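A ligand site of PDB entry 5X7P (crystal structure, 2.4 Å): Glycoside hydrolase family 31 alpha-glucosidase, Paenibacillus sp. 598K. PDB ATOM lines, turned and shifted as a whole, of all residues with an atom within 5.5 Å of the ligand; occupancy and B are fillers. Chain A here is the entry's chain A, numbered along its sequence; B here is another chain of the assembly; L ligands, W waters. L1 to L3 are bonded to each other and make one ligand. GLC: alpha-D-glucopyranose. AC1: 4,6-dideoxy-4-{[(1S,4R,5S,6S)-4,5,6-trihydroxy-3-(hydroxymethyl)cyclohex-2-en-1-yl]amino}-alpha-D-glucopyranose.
Water W2 bridges O2 of AC1 L3 and NE2 of Gln 176 of chain B.
The guanidinium group of Arg 456 is in salt-bridge range of the side-chain carboxylate of Asp 473 (3.8 Å). The side-chain carboxylate (OD1) of Asp 411 lies within salt-bridge range of the guanidinium group (NH1) of Arg 456 (3.4 Å). NH1 of Arg 456 lies close to NE2 of Gln 176 of chain B (3.3 Å). NZ of Lys 338 of chain B lies within salt-bridge range of OE1 of Glu 412, 3.2 Å away. The side-chain carboxylate (OD2) of Asp 411 lies within salt-bridge range of the side-chain amino group (NZ) of Lys 338 of chain B (2.7 Å). The side-chain amide nitrogen (ND2) of Asn 516 is in hydrogen-bond range of the backbone carbonyl oxygen (O) of Asp 473 (3.2 Å). NE2 of Gln 176 of chain B lies within hydrogen-bond range of OD2 of Asp 473 (2.8 Å). The side-chain carboxylate (OD1) of Asp 511 sits close to the indole nitrogen (NE1) of Trp 470 (3.4 Å).
Merely in contact with the ligand: Trp 409 (3.6 Å), Trp 470 (3.9 Å), Trp 486 (3.8 Å), Phe 515 (3.5 Å), Gln 176 of chain B (3.7 Å), Trp 266 of chain B (3.7 Å), Tyr 294 of chain B (3.3 Å) and Ile 336 of chain B (3.4 Å). Hydrophobic or aromatic side chains that line the ligand: Trp 409, Trp 470, Trp 486, Phe 515, His 547, Trp 266 of chain B, Tyr 294 of chain B and Ile 336 of chain B. Within 4 Å of the ligand: Trp 409, Asp 411, Glu 412, Arg 456, Trp 470, Asp 473, Trp 486, Phe 515, Asn 516, His 547, Gln 156 of chain B, Gln 176 of chain B, Trp 266 of chain B, Asp 293 of chain B, Tyr 294 of chain B, Ile 336 of chain B, Lys 338 of chain B, Gly 419 of chain B and Ser 420 of chain B.
OD2 of Asp 293 of chain B is in hydrogen-bond range of O4 of AC1 L3 (2.5 Å). The guanidinium group of Arg 456 is in hydrogen-bond range of an oxygen (O2B) of AC1 L3 (2.7 Å). An oxygen (O6B) of AC1 L3 is in hydrogen-bond range of the side-chain amino group of Lys 338 of chain B (2.7 Å). OD2 of Asp 473 lies within salt-bridge range of N4A of AC1 L3, at 3.0 Å. The side-chain carboxylate (OE2) of Glu 412 is in hydrogen-bond range of an oxygen (O3) of AC1 L3 (2.9 Å). An oxygen (O4) of AC1 L3 is in hydrogen-bond range of a ring nitrogen (NE2) of His 547 (2.9 Å). ND2 of Asn 516 is in hydrogen-bond range of O6 of GLC L2 (2.9 Å). N of Ser 420 of chain B is in hydrogen-bond range of O3 of GLC L1, 2.9 Å away. An oxygen (O3) of GLC L1 lies close to the backbone carbonyl oxygen of Gly 419 of chain B, 3.3 Å away. NE2 of Gln 156 of chain B sits close to O6 of GLC L1 (3.3 Å). The side-chain carboxylate of Asp 411 sits at hydrogen-bond distance from an oxygen (O2B) of AC1 L3, 3.3 Å away.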
ATOM      1  N   TYR A 373     -14.454 -24.360 -11.610  1.00  0.00           N
ATOM      2  CA  TYR A 373     -13.496 -24.584 -12.694  1.00  0.00           C
ATOM      3  C   TYR A 373     -12.320 -25.293 -12.090  1.00  0.00           C
ATOM      4  O   TYR A 373     -12.069 -25.144 -10.886  1.00  0.00           O
ATOM      5  CB  TYR A 373     -13.040 -23.252 -13.239  1.00  0.00           C
ATOM      6  CG  TYR A 373     -14.099 -22.417 -13.917  1.00  0.00           C
ATOM      7  CD1 TYR A 373     -14.872 -21.498 -13.215  1.00  0.00           C
ATOM      8  CD2 TYR A 373     -14.300 -22.527 -15.293  1.00  0.00           C
ATOM      9  CE1 TYR A 373     -15.840 -20.718 -13.866  1.00  0.00           C
ATOM     10  CE2 TYR A 373     -15.245 -21.760 -15.950  1.00  0.00           C
ATOM     11  CZ  TYR A 373     -16.022 -20.864 -15.247  1.00  0.00           C
ATOM     12  OH  TYR A 373     -16.947 -20.138 -15.971  1.00  0.00           O
ATOM     13  N   TRP A 409     -17.216 -13.267 -33.076  1.00  0.00           N
ATOM     14  CA  TRP A 409     -17.732 -12.962 -31.757  1.00  0.00           C
ATOM     15  C   TRP A 409     -16.553 -12.588 -30.873  1.00  0.00           C
ATOM     16  O   TRP A 409     -15.896 -13.438 -30.276  1.00  0.00           O
ATOM     17  CB  TRP A 409     -18.567 -14.154 -31.299  1.00  0.00           C
ATOM     18  CG  TRP A 409     -19.137 -14.139 -29.986  1.00  0.00           C
ATOM     19  CD1 TRP A 409     -19.280 -13.082 -29.146  1.00  0.00           C
ATOM     20  CD2 TRP A 409     -19.717 -15.254 -29.337  1.00  0.00           C
ATOM     21  NE1 TRP A 409     -19.875 -13.497 -27.976  1.00  0.00           N
ATOM     22  CE2 TRP A 409     -20.162 -14.831 -28.079  1.00  0.00           C
ATOM     23  CE3 TRP A 409     -19.862 -16.619 -29.692  1.00  0.00           C
ATOM     24  CZ2 TRP A 409     -20.769 -15.697 -27.160  1.00  0.00           C
ATOM     25  CZ3 TRP A 409     -20.453 -17.483 -28.780  1.00  0.00           C
ATOM     26  CH2 TRP A 409     -20.883 -17.013 -27.510  1.00  0.00           C
ATOM     27  N   ASP A 411     -15.042 -11.432 -27.930  1.00  0.00           N
ATOM     28  CA  ASP A 411     -15.429 -11.353 -26.526  1.00  0.00           C
ATOM     29  C   ASP A 411     -14.289 -10.766 -25.664  1.00  0.00           C
ATOM     30  O   ASP A 411     -13.121 -10.773 -26.052  1.00  0.00           O
ATOM     31  CB  ASP A 411     -15.843 -12.750 -26.074  1.00  0.00           C
ATOM     32  CG  ASP A 411     -16.387 -12.799 -24.666  1.00  0.00           C
ATOM     33  OD1 ASP A 411     -17.015 -11.843 -24.196  1.00  0.00           O
ATOM     34  OD2 ASP A 411     -16.172 -13.837 -24.021  1.00  0.00           O
ATOM     35  N   GLU A 412     -14.665 -10.199 -24.514  1.00  0.00           N
ATOM     36  CA  GLU A 412     -13.705  -9.830 -23.480  1.00  0.00           C
ATOM     37  C   GLU A 412     -12.589  -8.914 -24.009  1.00  0.00           C
ATOM     38  O   GLU A 412     -11.416  -9.104 -23.685  1.00  0.00           O
ATOM     39  CB  GLU A 412     -13.125 -11.106 -22.817  1.00  0.00           C
ATOM     40  CG  GLU A 412     -14.126 -11.856 -21.949  1.00  0.00           C
ATOM     41  CD  GLU A 412     -13.665 -13.228 -21.455  1.00  0.00           C
ATOM     42  OE1 GLU A 412     -12.840 -13.861 -22.111  1.00  0.00           O
ATOM     43  OE2 GLU A 412     -14.151 -13.707 -20.412  1.00  0.00           O
ATOM     44  N   ASP A 417     -11.007 -10.174 -15.739  1.00  0.00           N
ATOM     45  CA  ASP A 417     -11.443 -10.323 -14.330  1.00  0.00           C
ATOM     46  C   ASP A 417     -11.223 -11.779 -13.875  1.00  0.00           C
ATOM     47  O   ASP A 417     -12.056 -12.643 -14.070  1.00  0.00           O
ATOM     48  CB  ASP A 417     -12.927  -9.916 -14.231  1.00  0.00           C
ATOM     49  CG  ASP A 417     -13.357  -9.564 -12.802  1.00  0.00           C
ATOM     50  OD1 ASP A 417     -12.760 -10.090 -11.833  1.00  0.00           O
ATOM     51  OD2 ASP A 417     -14.321  -8.752 -12.670  1.00  0.00           O
ATOM     52  N   ARG A 456     -18.517  -6.601 -26.856  1.00  0.00           N
ATOM     53  CA  ARG A 456     -19.322  -6.161 -25.721  1.00  0.00           C
ATOM     54  C   ARG A 456     -18.927  -4.795 -25.111  1.00  0.00           C
ATOM     55  O   ARG A 456     -19.245  -4.486 -23.965  1.00  0.00           O
ATOM     56  CB  ARG A 456     -19.476  -7.305 -24.704  1.00  0.00           C
ATOM     57  CG  ARG A 456     -18.259  -7.537 -23.891  1.00  0.00           C
ATOM     58  CD  ARG A 456     -18.428  -8.751 -23.013  1.00  0.00           C
ATOM     59  NE  ARG A 456     -17.336  -8.711 -22.055  1.00  0.00           N
ATOM     60  CZ  ARG A 456     -17.053  -9.643 -21.169  1.00  0.00           C
ATOM     61  NH1 ARG A 456     -17.749 -10.797 -21.076  1.00  0.00           N
ATOM     62  NH2 ARG A 456     -16.023  -9.413 -20.382  1.00  0.00           N
ATOM     63  N   TRP A 470     -23.177  -6.249 -28.140  1.00  0.00           N
ATOM     64  CA  TRP A 470     -24.210  -6.961 -27.325  1.00  0.00           C
ATOM     65  C   TRP A 470     -24.097  -6.564 -25.864  1.00  0.00           C
ATOM     66  O   TRP A 470     -23.052  -6.134 -25.455  1.00  0.00           O
ATOM     67  CB  TRP A 470     -24.201  -8.470 -27.551  1.00  0.00           C
ATOM     68  CG  TRP A 470     -23.387  -9.323 -26.621  1.00  0.00           C
ATOM     69  CD1 TRP A 470     -23.836 -10.014 -25.531  1.00  0.00           C
ATOM     70  CD2 TRP A 470     -21.986  -9.671 -26.759  1.00  0.00           C
ATOM     71  NE1 TRP A 470     -22.801 -10.712 -24.945  1.00  0.00           N
ATOM     72  CE2 TRP A 470     -21.666 -10.536 -25.694  1.00  0.00           C
ATOM     73  CE3 TRP A 470     -20.974  -9.312 -27.677  1.00  0.00           C
ATOM     74  CZ2 TRP A 470     -20.393 -11.044 -25.508  1.00  0.00           C
ATOM     75  CZ3 TRP A 470     -19.694  -9.816 -27.503  1.00  0.00           C
ATOM     76  CH2 TRP A 470     -19.409 -10.679 -26.417  1.00  0.00           C
ATOM     77  N   GLY A 472     -23.728  -7.892 -22.979  1.00  0.00           N
ATOM     78  CA  GLY A 472     -22.938  -8.630 -22.010  1.00  0.00           C
ATOM     79  C   GLY A 472     -23.729  -9.683 -21.240  1.00  0.00           C
ATOM     80  O   GLY A 472     -24.788 -10.115 -21.667  1.00  0.00           O
ATOM     81  N   ASP A 473     -23.215 -10.053 -20.079  1.00  0.00           N
ATOM     82  CA  ASP A 473     -23.701 -11.200 -19.301  1.00  0.00           C
ATOM     83  C   ASP A 473     -24.910 -10.862 -18.433  1.00  0.00           C
ATOM     84  O   ASP A 473     -24.862 -10.937 -17.220  1.00  0.00           O
ATOM     85  CB  ASP A 473     -22.550 -11.724 -18.433  1.00  0.00           C
ATOM     86  CG  ASP A 473     -21.455 -12.375 -19.212  1.00  0.00           C
ATOM     87  OD1 ASP A 473     -21.715 -12.964 -20.310  1.00  0.00           O
ATOM     88  OD2 ASP A 473     -20.316 -12.347 -18.718  1.00  0.00           O
ATOM     89  N   TRP A 486     -27.206  -8.516  -8.699  1.00  0.00           N
ATOM     90  CA  TRP A 486     -25.887  -8.199  -9.294  1.00  0.00           C
ATOM     91  C   TRP A 486     -25.839  -8.114 -10.847  1.00  0.00           C
ATOM     92  O   TRP A 486     -24.771  -7.809 -11.418  1.00  0.00           O
ATOM     93  CB  TRP A 486     -24.786  -9.148  -8.764  1.00  0.00           C
ATOM     94  CG  TRP A 486     -25.153 -10.602  -8.692  1.00  0.00           C
ATOM     95  CD1 TRP A 486     -25.679 -11.269  -7.602  1.00  0.00           C
ATOM     96  CD2 TRP A 486     -25.039 -11.586  -9.738  1.00  0.00           C
ATOM     97  NE1 TRP A 486     -25.910 -12.566  -7.927  1.00  0.00           N
ATOM     98  CE2 TRP A 486     -25.497 -12.804  -9.209  1.00  0.00           C
ATOM     99  CE3 TRP A 486     -24.570 -11.544 -11.059  1.00  0.00           C
ATOM    100  CZ2 TRP A 486     -25.535 -13.988  -9.965  1.00  0.00           C
ATOM    101  CZ3 TRP A 486     -24.587 -12.723 -11.809  1.00  0.00           C
ATOM    102  CH2 TRP A 486     -25.069 -13.931 -11.258  1.00  0.00           C
ATOM    103  N   ASP A 511     -28.445 -10.994 -25.071  1.00  0.00           N
ATOM    104  CA  ASP A 511     -28.574 -12.431 -24.877  1.00  0.00           C
ATOM    105  C   ASP A 511     -30.030 -12.704 -24.556  1.00  0.00           C
ATOM    106  O   ASP A 511     -30.438 -12.591 -23.405  1.00  0.00           O
ATOM    107  CB  ASP A 511     -27.709 -12.904 -23.707  1.00  0.00           C
ATOM    108  CG  ASP A 511     -26.196 -12.866 -23.983  1.00  0.00           C
ATOM    109  OD1 ASP A 511     -25.725 -12.503 -25.083  1.00  0.00           O
ATOM    110  OD2 ASP A 511     -25.452 -13.225 -23.049  1.00  0.00           O
ATOM    111  N   PHE A 515     -28.046 -14.648 -19.663  1.00  0.00           N
ATOM    112  CA  PHE A 515     -26.825 -15.414 -19.516  1.00  0.00           C
ATOM    113  C   PHE A 515     -26.656 -15.959 -18.105  1.00  0.00           C
ATOM    114  O   PHE A 515     -26.367 -17.135 -17.955  1.00  0.00           O
ATOM    115  CB  PHE A 515     -25.613 -14.558 -19.845  1.00  0.00           C
ATOM    116  CG  PHE A 515     -24.320 -15.354 -19.891  1.00  0.00           C
ATOM    117  CD1 PHE A 515     -23.995 -16.130 -21.024  1.00  0.00           C
ATOM    118  CD2 PHE A 515     -23.457 -15.371 -18.803  1.00  0.00           C
ATOM    119  CE1 PHE A 515     -22.810 -16.845 -21.058  1.00  0.00           C
ATOM    120  CE2 PHE A 515     -22.308 -16.142 -18.815  1.00  0.00           C
ATOM    121  CZ  PHE A 515     -21.970 -16.852 -19.948  1.00  0.00           C
ATOM    122  N   ASN A 516     -26.816 -15.126 -17.093  1.00  0.00           N
ATOM    123  CA  ASN A 516     -26.509 -15.503 -15.722  1.00  0.00           C
ATOM    124  C   ASN A 516     -27.709 -15.907 -14.859  1.00  0.00           C
ATOM    125  O   ASN A 516     -28.784 -15.348 -14.965  1.00  0.00           O
ATOM    126  CB  ASN A 516     -25.827 -14.363 -14.995  1.00  0.00           C
ATOM    127  CG  ASN A 516     -24.313 -14.434 -15.092  1.00  0.00           C
ATOM    128  OD1 ASN A 516     -23.702 -15.501 -14.949  1.00  0.00           O
ATOM    129  ND2 ASN A 516     -23.702 -13.267 -15.297  1.00  0.00           N
ATOM    130  N   ARG A 545     -30.653 -12.564 -31.271  1.00  0.00           N
ATOM    131  CA  ARG A 545     -29.926 -13.767 -30.891  1.00  0.00           C
ATOM    132  C   ARG A 545     -30.269 -14.240 -29.488  1.00  0.00           C
ATOM    133  O   ARG A 545     -30.452 -13.421 -28.581  1.00  0.00           O
ATOM    134  CB  ARG A 545     -28.436 -13.494 -30.950  1.00  0.00           C
ATOM    135  CG  ARG A 545     -27.991 -12.251 -30.168  1.00  0.00           C
ATOM    136  CD  ARG A 545     -26.505 -11.887 -30.369  1.00  0.00           C
ATOM    137  NE  ARG A 545     -25.617 -12.655 -29.517  1.00  0.00           N
ATOM    138  CZ  ARG A 545     -25.514 -12.503 -28.201  1.00  0.00           C
ATOM    139  NH1 ARG A 545     -26.285 -11.626 -27.535  1.00  0.00           N
ATOM    140  NH2 ARG A 545     -24.661 -13.269 -27.509  1.00  0.00           N
ATOM    141  N   HIS A 547     -28.692 -16.564 -26.292  1.00  0.00           N
ATOM    142  CA  HIS A 547     -27.455 -17.062 -25.741  1.00  0.00           C
ATOM    143  C   HIS A 547     -27.746 -17.542 -24.349  1.00  0.00           C
ATOM    144  O   HIS A 547     -28.808 -17.263 -23.790  1.00  0.00           O
ATOM    145  CB  HIS A 547     -26.352 -15.990 -25.774  1.00  0.00           C
ATOM    146  CG  HIS A 547     -24.994 -16.505 -25.415  1.00  0.00           C
ATOM    147  ND1 HIS A 547     -24.605 -17.803 -25.653  1.00  0.00           N
ATOM    148  CD2 HIS A 547     -23.922 -15.892 -24.848  1.00  0.00           C
ATOM    149  CE1 HIS A 547     -23.372 -17.986 -25.229  1.00  0.00           C
ATOM    150  NE2 HIS A 547     -22.932 -16.835 -24.748  1.00  0.00           N
ATOM    151  N   GLY A 548     -26.851 -18.344 -23.819  1.00  0.00           N
ATOM    152  CA  GLY A 548     -26.915 -18.706 -22.433  1.00  0.00           C
ATOM    153  C   GLY A 548     -25.602 -19.233 -21.942  1.00  0.00           C
ATOM    154  O   GLY A 548     -24.639 -19.351 -22.696  1.00  0.00           O
ATOM    155  N   ASN A 549     -25.604 -19.616 -20.668  1.00  0.00           N
ATOM    156  CA  ASN A 549     -24.388 -20.064 -20.005  1.00  0.00           C
ATOM    157  C   ASN A 549     -24.041 -21.506 -20.461  1.00  0.00           C
ATOM    158  O   ASN A 549     -24.754 -22.106 -21.251  1.00  0.00           O
ATOM    159  CB  ASN A 549     -24.566 -19.972 -18.490  1.00  0.00           C
ATOM    160  CG  ASN A 549     -23.304 -19.547 -17.772  1.00  0.00           C
ATOM    161  OD1 ASN A 549     -22.212 -19.786 -18.268  1.00  0.00           O
ATOM    162  ND2 ASN A 549     -23.448 -18.935 -16.600  1.00  0.00           N
ATOM    163  N   GLN B 156     -23.535  -5.228 -15.127  1.00  0.00           N
ATOM    164  CA  GLN B 156     -23.250  -5.258 -13.682  1.00  0.00           C
ATOM    165  C   GLN B 156     -23.641  -3.983 -12.988  1.00  0.00           C
ATOM    166  O   GLN B 156     -23.246  -3.791 -11.853  1.00  0.00           O
ATOM    167  CB  GLN B 156     -21.747  -5.515 -13.422  1.00  0.00           C
ATOM    168  CG  GLN B 156     -21.233  -6.832 -13.979  1.00  0.00           C
ATOM    169  CD  GLN B 156     -19.729  -6.967 -13.920  1.00  0.00           C
ATOM    170  OE1 GLN B 156     -19.033  -6.056 -13.456  1.00  0.00           O
ATOM    171  NE2 GLN B 156     -19.212  -8.106 -14.403  1.00  0.00           N
ATOM    172  N   GLN B 176     -18.617  -5.214 -20.418  1.00  0.00           N
ATOM    173  CA  GLN B 176     -19.826  -5.976 -20.141  1.00  0.00           C
ATOM    174  C   GLN B 176     -21.069  -5.249 -20.724  1.00  0.00           C
ATOM    175  O   GLN B 176     -22.106  -5.048 -20.074  1.00  0.00           O
ATOM    176  CB  GLN B 176     -19.929  -6.269 -18.625  1.00  0.00           C
ATOM    177  CG  GLN B 176     -19.096  -7.466 -18.124  1.00  0.00           C
ATOM    178  CD  GLN B 176     -19.624  -8.831 -18.587  1.00  0.00           C
ATOM    179  OE1 GLN B 176     -20.577  -8.880 -19.346  1.00  0.00           O
ATOM    180  NE2 GLN B 176     -18.976  -9.909 -18.173  1.00  0.00           N
ATOM    181  N   TRP B 266     -22.842 -22.260 -25.931  1.00  0.00           N
ATOM    182  CA  TRP B 266     -21.643 -22.767 -25.260  1.00  0.00           C
ATOM    183  C   TRP B 266     -22.017 -24.148 -24.710  1.00  0.00           C
ATOM    184  O   TRP B 266     -22.955 -24.267 -23.898  1.00  0.00           O
ATOM    185  CB  TRP B 266     -21.281 -21.802 -24.129  1.00  0.00           C
ATOM    186  CG  TRP B 266     -19.982 -22.046 -23.438  1.00  0.00           C
ATOM    187  CD1 TRP B 266     -18.974 -22.869 -23.829  1.00  0.00           C
ATOM    188  CD2 TRP B 266     -19.555 -21.427 -22.235  1.00  0.00           C
ATOM    189  NE1 TRP B 266     -17.942 -22.812 -22.922  1.00  0.00           N
ATOM    190  CE2 TRP B 266     -18.275 -21.921 -21.937  1.00  0.00           C
ATOM    191  CE3 TRP B 266     -20.144 -20.503 -21.362  1.00  0.00           C
ATOM    192  CZ2 TRP B 266     -17.566 -21.519 -20.806  1.00  0.00           C
ATOM    193  CZ3 TRP B 266     -19.436 -20.082 -20.244  1.00  0.00           C
ATOM    194  CH2 TRP B 266     -18.153 -20.591 -19.974  1.00  0.00           C
ATOM    195  N   ASP B 293     -19.173 -21.108 -29.137  1.00  0.00           N
ATOM    196  CA  ASP B 293     -18.278 -20.670 -28.050  1.00  0.00           C
ATOM    197  C   ASP B 293     -16.937 -21.462 -28.116  1.00  0.00           C
ATOM    198  O   ASP B 293     -16.561 -21.938 -29.174  1.00  0.00           O
ATOM    199  CB  ASP B 293     -19.002 -20.797 -26.682  1.00  0.00           C
ATOM    200  CG  ASP B 293     -18.529 -19.741 -25.629  1.00  0.00           C
ATOM    201  OD1 ASP B 293     -17.331 -19.662 -25.298  1.00  0.00           O
ATOM    202  OD2 ASP B 293     -19.381 -18.994 -25.090  1.00  0.00           O
ATOM    203  N   TYR B 294     -16.209 -21.575 -27.010  1.00  0.00           N
ATOM    204  CA  TYR B 294     -14.922 -22.305 -26.923  1.00  0.00           C
ATOM    205  C   TYR B 294     -14.931 -23.654 -27.643  1.00  0.00           C
ATOM    206  O   TYR B 294     -13.907 -24.089 -28.189  1.00  0.00           O
ATOM    207  CB  TYR B 294     -14.553 -22.571 -25.459  1.00  0.00           C
ATOM    208  CG  TYR B 294     -14.026 -21.403 -24.600  1.00  0.00           C
ATOM    209  CD1 TYR B 294     -12.777 -20.846 -24.835  1.00  0.00           C
ATOM    210  CD2 TYR B 294     -14.739 -20.946 -23.514  1.00  0.00           C
ATOM    211  CE1 TYR B 294     -12.251 -19.833 -24.026  1.00  0.00           C
ATOM    212  CE2 TYR B 294     -14.226 -19.927 -22.702  1.00  0.00           C
ATOM    213  CZ  TYR B 294     -12.978 -19.378 -22.957  1.00  0.00           C
ATOM    214  OH  TYR B 294     -12.465 -18.372 -22.149  1.00  0.00           O
ATOM    215  N   ILE B 336     -16.374 -17.647 -31.425  1.00  0.00           N
ATOM    216  CA  ILE B 336     -15.972 -16.699 -30.368  1.00  0.00           C
ATOM    217  C   ILE B 336     -14.455 -16.505 -30.439  1.00  0.00           C
ATOM    218  O   ILE B 336     -13.713 -17.447 -30.737  1.00  0.00           O
ATOM    219  CB  ILE B 336     -16.455 -17.126 -28.931  1.00  0.00           C
ATOM    220  CG1 ILE B 336     -16.362 -15.911 -27.978  1.00  0.00           C
ATOM    221  CG2 ILE B 336     -15.692 -18.349 -28.379  1.00  0.00           C
ATOM    222  CD1 ILE B 336     -16.927 -16.129 -26.592  1.00  0.00           C
ATOM    223  N   LYS B 338     -11.193 -14.427 -28.260  1.00  0.00           N
ATOM    224  CA  LYS B 338     -10.680 -13.802 -27.060  1.00  0.00           C
ATOM    225  C   LYS B 338      -9.391 -13.112 -27.458  1.00  0.00           C
ATOM    226  O   LYS B 338      -8.573 -13.729 -28.115  1.00  0.00           O
ATOM    227  CB  LYS B 338     -10.346 -14.885 -26.033  1.00  0.00           C
ATOM    228  CG  LYS B 338     -11.432 -15.900 -25.810  1.00  0.00           C
ATOM    229  CD  LYS B 338     -12.663 -15.272 -25.167  1.00  0.00           C
ATOM    230  CE  LYS B 338     -13.701 -16.360 -24.872  1.00  0.00           C
ATOM    231  NZ  LYS B 338     -14.602 -15.961 -23.766  1.00  0.00           N
ATOM    232  N   SER B 418     -16.728 -19.196  -4.884  1.00  0.00           N
ATOM    233  CA  SER B 418     -16.751 -19.607  -6.283  1.00  0.00           C
ATOM    234  C   SER B 418     -17.904 -19.000  -7.080  1.00  0.00           C
ATOM    235  O   SER B 418     -19.052 -19.488  -7.054  1.00  0.00           O
ATOM    236  CB  SER B 418     -16.780 -21.130  -6.348  1.00  0.00           C
ATOM    237  OG  SER B 418     -16.483 -21.600  -7.652  1.00  0.00           O
ATOM    238  N   GLY B 419     -17.596 -17.936  -7.804  1.00  0.00           N
ATOM    239  CA  GLY B 419     -18.559 -17.285  -8.649  1.00  0.00           C
ATOM    240  C   GLY B 419     -19.664 -16.714  -7.818  1.00  0.00           C
ATOM    241  O   GLY B 419     -19.401 -15.953  -6.889  1.00  0.00           O
ATOM    242  N   SER B 420     -20.909 -17.089  -8.109  1.00  0.00           N
ATOM    243  CA  SER B 420     -22.036 -16.677  -7.256  1.00  0.00           C
ATOM    244  C   SER B 420     -22.098 -17.523  -5.976  1.00  0.00           C
ATOM    245  O   SER B 420     -22.665 -17.041  -4.970  1.00  0.00           O
ATOM    246  CB  SER B 420     -23.389 -16.682  -8.019  1.00  0.00           C
ATOM    247  OG  SER B 420     -24.127 -17.886  -7.872  1.00  0.00           O
ATOM    248  N   ALA B 421     -21.518 -18.735  -5.992  1.00  0.00           N
ATOM    249  CA  ALA B 421     -21.567 -19.603  -4.820  1.00  0.00           C
ATOM    250  C   ALA B 421     -20.615 -19.195  -3.660  1.00  0.00           C
ATOM    251  O   ALA B 421     -19.400 -19.254  -3.783  1.00  0.00           O
ATOM    252  CB  ALA B 421     -21.325 -21.033  -5.254  1.00  0.00           C
HETATM  253  C1  GLC L   1     -21.374 -10.725  -8.093  1.00  0.00           C
HETATM  254  C2  GLC L   1     -21.723 -12.219  -8.063  1.00  0.00           C
HETATM  255  C3  GLC L   1     -20.790 -13.048  -8.949  1.00  0.00           C
HETATM  256  C4  GLC L   1     -20.687 -12.440 -10.359  1.00  0.00           C
HETATM  257  C5  GLC L   1     -20.239 -10.969 -10.263  1.00  0.00           C
HETATM  258  C6  GLC L   1     -20.194 -10.303 -11.635  1.00  0.00           C
HETATM  259  O1  GLC L   1     -20.199 -10.515  -7.357  1.00  0.00           O
HETATM  260  O2  GLC L   1     -21.735 -12.687  -6.722  1.00  0.00           O
HETATM  261  O3  GLC L   1     -21.341 -14.361  -9.096  1.00  0.00           O
HETATM  262  O4  GLC L   1     -19.798 -13.223 -11.193  1.00  0.00           O
HETATM  263  O5  GLC L   1     -21.158 -10.248  -9.439  1.00  0.00           O
HETATM  264  O6  GLC L   1     -20.555  -8.924 -11.557  1.00  0.00           O
HETATM  265  C1  GLC L   2     -20.412 -14.141 -12.120  1.00  0.00           C
HETATM  266  C2  GLC L   2     -19.410 -15.245 -12.474  1.00  0.00           C
HETATM  267  C3  GLC L   2     -18.233 -14.713 -13.295  1.00  0.00           C
HETATM  268  C4  GLC L   2     -18.729 -14.014 -14.557  1.00  0.00           C
HETATM  269  C5  GLC L   2     -19.737 -12.926 -14.117  1.00  0.00           C
HETATM  270  C6  GLC L   2     -20.345 -12.181 -15.294  1.00  0.00           C
HETATM  271  O2  GLC L   2     -18.909 -15.822 -11.280  1.00  0.00           O
HETATM  272  O3  GLC L   2     -17.390 -15.808 -13.636  1.00  0.00           O
HETATM  273  O4  GLC L   2     -17.647 -13.412 -15.352  1.00  0.00           O
HETATM  274  O5  GLC L   2     -20.812 -13.507 -13.347  1.00  0.00           O
HETATM  275  O6  GLC L   2     -20.913 -13.199 -16.132  1.00  0.00           O
HETATM  276  C1  AC1 L   3     -16.713 -14.259 -16.044  1.00  0.00           C
HETATM  277  O2  AC1 L   3     -15.463 -12.271 -16.617  1.00  0.00           O
HETATM  278  C2  AC1 L   3     -16.014 -13.477 -17.149  1.00  0.00           C
HETATM  279  C4A AC1 L   3     -19.345 -16.197 -23.348  1.00  0.00           C
HETATM  280  C3  AC1 L   3     -17.030 -13.183 -18.264  1.00  0.00           C
HETATM  281  O3  AC1 L   3     -16.412 -12.356 -19.254  1.00  0.00           O
HETATM  282  C4  AC1 L   3     -17.547 -14.524 -18.817  1.00  0.00           C
HETATM  283  N4A AC1 L   3     -18.451 -14.284 -19.960  1.00  0.00           N
HETATM  284  C5  AC1 L   3     -18.181 -15.401 -17.695  1.00  0.00           C
HETATM  285  O5  AC1 L   3     -17.309 -15.469 -16.580  1.00  0.00           O
HETATM  286  C6  AC1 L   3     -18.490 -16.864 -18.044  1.00  0.00           C
HETATM  287  C1B AC1 L   3     -17.978 -14.408 -21.346  1.00  0.00           C
HETATM  288  C2B AC1 L   3     -18.962 -13.878 -22.415  1.00  0.00           C
HETATM  289  O2B AC1 L   3     -19.486 -12.551 -22.077  1.00  0.00           O
HETATM  290  C3B AC1 L   3     -20.018 -14.948 -22.763  1.00  0.00           C
HETATM  291  O3B AC1 L   3     -20.929 -14.474 -23.774  1.00  0.00           O
HETATM  292  O4  AC1 L   3     -20.340 -17.229 -23.526  1.00  0.00           O
HETATM  293  C5B AC1 L   3     -18.193 -16.662 -22.481  1.00  0.00           C
HETATM  294  C7B AC1 L   3     -17.607 -15.871 -21.569  1.00  0.00           C
HETATM  295  C6B AC1 L   3     -17.582 -18.019 -22.617  1.00  0.00           C
HETATM  296  O6B AC1 L   3     -16.578 -17.814 -23.614  1.00  0.00           O
HETATM  297  O   HOH W   1     -23.060 -12.740 -22.770  1.00  0.00           O
HETATM  298  O   HOH W   2     -17.033 -10.315 -16.030  1.00  0.00           O
